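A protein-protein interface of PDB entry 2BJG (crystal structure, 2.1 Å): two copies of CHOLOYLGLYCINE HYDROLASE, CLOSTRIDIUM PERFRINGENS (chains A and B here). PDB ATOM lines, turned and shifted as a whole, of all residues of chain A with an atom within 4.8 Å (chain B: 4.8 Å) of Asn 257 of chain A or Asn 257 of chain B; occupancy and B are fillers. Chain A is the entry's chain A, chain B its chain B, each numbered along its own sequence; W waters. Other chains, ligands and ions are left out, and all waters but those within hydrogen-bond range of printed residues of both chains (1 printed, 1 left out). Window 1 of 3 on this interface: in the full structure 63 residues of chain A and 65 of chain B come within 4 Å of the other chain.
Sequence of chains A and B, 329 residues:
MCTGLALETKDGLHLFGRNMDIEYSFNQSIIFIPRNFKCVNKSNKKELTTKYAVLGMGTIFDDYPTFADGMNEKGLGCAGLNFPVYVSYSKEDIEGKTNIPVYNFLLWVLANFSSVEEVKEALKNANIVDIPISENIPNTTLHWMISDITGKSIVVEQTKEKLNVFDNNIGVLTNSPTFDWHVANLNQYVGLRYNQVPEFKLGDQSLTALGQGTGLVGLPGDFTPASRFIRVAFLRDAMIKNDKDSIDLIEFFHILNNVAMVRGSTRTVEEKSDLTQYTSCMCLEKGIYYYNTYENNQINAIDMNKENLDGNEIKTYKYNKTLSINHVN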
ATOM      1  N   PHE A 253      22.639  17.192 -13.790  1.00  0.00           N
ATOM      2  CA  PHE A 253      22.544  16.599 -12.456  1.00  0.00           C
ATOM      3  C   PHE A 253      21.094  16.396 -12.003  1.00  0.00           C
ATOM      4  O   PHE A 253      20.783  15.392 -11.365  1.00  0.00           O
ATOM      5  CB  PHE A 253      23.350  17.418 -11.442  1.00  0.00           C
ATOM      6  CG  PHE A 253      24.843  17.204 -11.540  1.00  0.00           C
ATOM      7  CD1 PHE A 253      25.481  16.265 -10.725  1.00  0.00           C
ATOM      8  CD2 PHE A 253      25.610  17.928 -12.454  1.00  0.00           C
ATOM      9  CE1 PHE A 253      26.860  16.060 -10.810  1.00  0.00           C
ATOM     10  CE2 PHE A 253      26.988  17.727 -12.547  1.00  0.00           C
ATOM     11  CZ  PHE A 253      27.612  16.791 -11.729  1.00  0.00           C
ATOM     12  N   HIS A 254      20.208  17.330 -12.353  1.00  0.00           N
ATOM     13  CA  HIS A 254      18.774  17.171 -12.073  1.00  0.00           C
ATOM     14  C   HIS A 254      18.181  15.919 -12.726  1.00  0.00           C
ATOM     15  O   HIS A 254      17.437  15.176 -12.088  1.00  0.00           O
ATOM     16  CB  HIS A 254      17.988  18.417 -12.484  1.00  0.00           C
ATOM     17  CG  HIS A 254      18.144  19.559 -11.534  1.00  0.00           C
ATOM     18  ND1 HIS A 254      17.559  19.570 -10.285  1.00  0.00           N
ATOM     19  CD2 HIS A 254      18.830  20.721 -11.638  1.00  0.00           C
ATOM     20  CE1 HIS A 254      17.875  20.692  -9.663  1.00  0.00           C
ATOM     21  NE2 HIS A 254      18.646  21.406 -10.461  1.00  0.00           N
ATOM     22  N   ILE A 255      18.531  15.676 -13.987  1.00  0.00           N
ATOM     23  CA  ILE A 255      18.065  14.472 -14.684  1.00  0.00           C
ATOM     24  C   ILE A 255      18.543  13.194 -13.979  1.00  0.00           C
ATOM     25  O   ILE A 255      17.726  12.327 -13.650  1.00  0.00           O
ATOM     26  CB  ILE A 255      18.459  14.466 -16.177  1.00  0.00           C
ATOM     27  CG1 ILE A 255      17.752  15.603 -16.928  1.00  0.00           C
ATOM     28  CG2 ILE A 255      18.102  13.121 -16.820  1.00  0.00           C
ATOM     29  CD1 ILE A 255      18.411  15.985 -18.271  1.00  0.00           C
ATOM     30  N   LEU A 256      19.848  13.098 -13.727  1.00  0.00           N
ATOM     31  CA  LEU A 256      20.428  11.902 -13.100  1.00  0.00           C
ATOM     32  C   LEU A 256      20.017  11.678 -11.634  1.00  0.00           C
ATOM     33  O   LEU A 256      19.964  10.527 -11.177  1.00  0.00           O
ATOM     34  CB  LEU A 256      21.956  11.862 -13.273  1.00  0.00           C
ATOM     35  CG  LEU A 256      22.470  11.603 -14.702  1.00  0.00           C
ATOM     36  CD1 LEU A 256      23.981  11.426 -14.723  1.00  0.00           C
ATOM     37  CD2 LEU A 256      21.791  10.367 -15.326  1.00  0.00           C
ATOM     38  N   ASN A 257      19.713  12.763 -10.915  1.00  0.00           N
ATOM     39  CA  ASN A 257      19.177  12.685  -9.547  1.00  0.00           C
ATOM     40  C   ASN A 257      17.877  11.894  -9.459  1.00  0.00           C
ATOM     41  O   ASN A 257      17.633  11.201  -8.468  1.00  0.00           O
ATOM     42  CB  ASN A 257      18.924  14.082  -8.965  1.00  0.00           C
ATOM     43  CG  ASN A 257      20.194  14.774  -8.496  1.00  0.00           C
ATOM     44  OD1 ASN A 257      21.312  14.255  -8.641  1.00  0.00           O
ATOM     45  ND2 ASN A 257      20.027  15.966  -7.934  1.00  0.00           N
ATOM     46  N   ASN A 258      17.044  12.015 -10.493  1.00  0.00           N
ATOM     47  CA  ASN A 258      15.747  11.340 -10.537  1.00  0.00           C
ATOM     48  C   ASN A 258      15.865   9.815 -10.566  1.00  0.00           C
ATOM     49  O   ASN A 258      14.963   9.107 -10.102  1.00  0.00           O
ATOM     50  CB  ASN A 258      14.926  11.817 -11.741  1.00  0.00           C
ATOM     51  CG  ASN A 258      13.563  11.156 -11.813  1.00  0.00           C
ATOM     52  OD1 ASN A 258      13.359  10.215 -12.580  1.00  0.00           O
ATOM     53  ND2 ASN A 258      12.625  11.631 -10.996  1.00  0.00           N
ATOM     54  N   VAL A 259      16.968   9.323 -11.122  1.00  0.00           N
ATOM     55  CA  VAL A 259      17.224   7.882 -11.196  1.00  0.00           C
ATOM     56  C   VAL A 259      18.340   7.419 -10.242  1.00  0.00           C
ATOM     57  O   VAL A 259      18.828   6.289 -10.340  1.00  0.00           O
ATOM     58  CB  VAL A 259      17.512   7.417 -12.648  1.00  0.00           C
ATOM     59  CG1 VAL A 259      16.251   7.499 -13.497  1.00  0.00           C
ATOM     60  CG2 VAL A 259      18.656   8.221 -13.280  1.00  0.00           C
ATOM     61  N   ALA A 260      18.724   8.290  -9.312  1.00  0.00           N
ATOM     62  CA  ALA A 260      19.746   7.965  -8.315  1.00  0.00           C
ATOM     63  C   ALA A 260      19.188   7.072  -7.209  1.00  0.00           C
ATOM     64  O   ALA A 260      18.047   7.262  -6.763  1.00  0.00           O
ATOM     65  CB  ALA A 260      20.347   9.234  -7.729  1.00  0.00           C
ATOM     66  N   PHE B 253      18.458  15.154   1.817  1.00  0.00           N
ATOM     67  CA  PHE B 253      18.456  15.684   0.458  1.00  0.00           C
ATOM     68  C   PHE B 253      18.318  14.583  -0.595  1.00  0.00           C
ATOM     69  O   PHE B 253      17.643  14.782  -1.600  1.00  0.00           O
ATOM     70  CB  PHE B 253      19.694  16.560   0.210  1.00  0.00           C
ATOM     71  CG  PHE B 253      19.600  17.933   0.835  1.00  0.00           C
ATOM     72  CD1 PHE B 253      19.145  19.019   0.091  1.00  0.00           C
ATOM     73  CD2 PHE B 253      19.957  18.136   2.168  1.00  0.00           C
ATOM     74  CE1 PHE B 253      19.053  20.292   0.661  1.00  0.00           C
ATOM     75  CE2 PHE B 253      19.866  19.404   2.754  1.00  0.00           C
ATOM     76  CZ  PHE B 253      19.407  20.484   1.998  1.00  0.00           C
ATOM     77  N   HIS B 254      18.939  13.426  -0.352  1.00  0.00           N
ATOM     78  CA  HIS B 254      18.778  12.256  -1.226  1.00  0.00           C
ATOM     79  C   HIS B 254      17.326  11.791  -1.346  1.00  0.00           C
ATOM     80  O   HIS B 254      16.861  11.453  -2.442  1.00  0.00           O
ATOM     81  CB  HIS B 254      19.672  11.098  -0.772  1.00  0.00           C
ATOM     82  CG  HIS B 254      21.115  11.283  -1.121  1.00  0.00           C
ATOM     83  ND1 HIS B 254      21.584  11.195  -2.412  1.00  0.00           N
ATOM     84  CD2 HIS B 254      22.194  11.548  -0.349  1.00  0.00           C
ATOM     85  CE1 HIS B 254      22.889  11.408  -2.424  1.00  0.00           C
ATOM     86  NE2 HIS B 254      23.284  11.624  -1.184  1.00  0.00           N
ATOM     87  N   ILE B 255      16.613  11.769  -0.223  1.00  0.00           N
ATOM     88  CA  ILE B 255      15.197  11.396  -0.233  1.00  0.00           C
ATOM     89  C   ILE B 255      14.376  12.386  -1.071  1.00  0.00           C
ATOM     90  O   ILE B 255      13.640  11.979  -1.968  1.00  0.00           O
ATOM     91  CB  ILE B 255      14.612  11.249   1.198  1.00  0.00           C
ATOM     92  CG1 ILE B 255      15.274  10.076   1.938  1.00  0.00           C
ATOM     93  CG2 ILE B 255      13.099  11.046   1.136  1.00  0.00           C
ATOM     94  CD1 ILE B 255      15.129  10.122   3.457  1.00  0.00           C
ATOM     95  N   LEU B 256      14.521  13.679  -0.787  1.00  0.00           N
ATOM     96  CA  LEU B 256      13.741  14.708  -1.480  1.00  0.00           C
ATOM     97  C   LEU B 256      14.110  14.891  -2.954  1.00  0.00           C
ATOM     98  O   LEU B 256      13.257  15.282  -3.750  1.00  0.00           O
ATOM     99  CB  LEU B 256      13.760  16.047  -0.720  1.00  0.00           C
ATOM    100  CG  LEU B 256      12.992  16.089   0.607  1.00  0.00           C
ATOM    101  CD1 LEU B 256      13.008  17.485   1.200  1.00  0.00           C
ATOM    102  CD2 LEU B 256      11.548  15.605   0.436  1.00  0.00           C
ATOM    103  N   ASN B 257      15.361  14.595  -3.314  1.00  0.00           N
ATOM    104  CA  ASN B 257      15.797  14.590  -4.726  1.00  0.00           C
ATOM    105  C   ASN B 257      14.994  13.624  -5.602  1.00  0.00           C
ATOM    106  O   ASN B 257      14.724  13.908  -6.770  1.00  0.00           O
ATOM    107  CB  ASN B 257      17.284  14.222  -4.850  1.00  0.00           C
ATOM    108  CG  ASN B 257      18.217  15.372  -4.505  1.00  0.00           C
ATOM    109  OD1 ASN B 257      17.785  16.458  -4.098  1.00  0.00           O
ATOM    110  ND2 ASN B 257      19.521  15.128  -4.652  1.00  0.00           N
ATOM    111  N   ASN B 258      14.631  12.474  -5.035  1.00  0.00           N
ATOM    112  CA  ASN B 258      13.863  11.458  -5.762  1.00  0.00           C
ATOM    113  C   ASN B 258      12.476  11.951  -6.208  1.00  0.00           C
ATOM    114  O   ASN B 258      11.939  11.479  -7.212  1.00  0.00           O
ATOM    115  CB  ASN B 258      13.727  10.189  -4.917  1.00  0.00           C
ATOM    116  CG  ASN B 258      12.936   9.104  -5.622  1.00  0.00           C
ATOM    117  OD1 ASN B 258      11.752   8.909  -5.347  1.00  0.00           O
ATOM    118  ND2 ASN B 258      13.579   8.405  -6.547  1.00  0.00           N
ATOM    119  N   VAL B 259      11.909  12.894  -5.459  1.00  0.00           N
ATOM    120  CA  VAL B 259      10.587  13.453  -5.768  1.00  0.00           C
ATOM    121  C   VAL B 259      10.657  14.911  -6.247  1.00  0.00           C
ATOM    122  O   VAL B 259       9.637  15.608  -6.296  1.00  0.00           O
ATOM    123  CB  VAL B 259       9.598  13.321  -4.578  1.00  0.00           C
ATOM    124  CG1 VAL B 259       9.232  11.853  -4.343  1.00  0.00           C
ATOM    125  CG2 VAL B 259      10.162  13.956  -3.310  1.00  0.00           C
ATOM    126  N   ALA B 260      11.863  15.354  -6.607  1.00  0.00           N
ATOM    127  CA  ALA B 260      12.068  16.693  -7.157  1.00  0.00           C
ATOM    128  C   ALA B 260      11.639  16.784  -8.624  1.00  0.00           C
ATOM    129  O   ALA B 260      11.875  15.861  -9.412  1.00  0.00           O
ATOM    130  CB  ALA B 260      13.525  17.113  -6.999  1.00  0.00           C
HETATM  131  O   HOH W   1      16.402   9.354  -6.831  1.00  0.00           O
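Asn 257 of chain A touches its own counterpart, Asn 257 of chain B.
Asn 258 of chain B touches its own counterpart, Asn 258 of chain A.
Of the 8 printed residues of chain B, 2 touch a printed residue of chain A.
Among the printed residues, 2 pairs touch across the chains.
Among the printed residues, no Asp or Glu carboxylate lies within 4 Å of a Lys or Arg side-chain nitrogen of the other chain.
ND2 of Asn 257 of chain B sits close to ND2 of Asn 257 of chain A (3.4 Å).
The side-chain amide oxygen (OD1) of Asn 257 of chain A lies close to the backbone carbonyl oxygen (O) of Phe 253 of chain A (3.0 Å).
The backbone carbonyl oxygen of Phe 253 of chain B lies close to the side-chain amide oxygen of Asn 257 of chain B (3.0 Å).
Among the printed residues, merely in contact across the chains: Asn 258 of chain A with Asn 258 of chain B.
Asn 257 of chain A touches just one residue of chain B: Asn 257 (3.4 Å).
Of chain A, only Asn 257 comes within 4 Å of Asn 257 of chain B.
Of the printed residues of chain A, Asn 258 of chain B touches Asn 258.
Of the printed residues of chain B, Asn 258 of chain A touches Asn 258 (3.8 Å).
His 254 of chain A touches none of the printed residues of chain B.
Water W1 lies within hydrogen-bond range of O of Ala 260 of chain A, O of Asn 257 of chain A and ND2 of Asn 258 of chain B.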
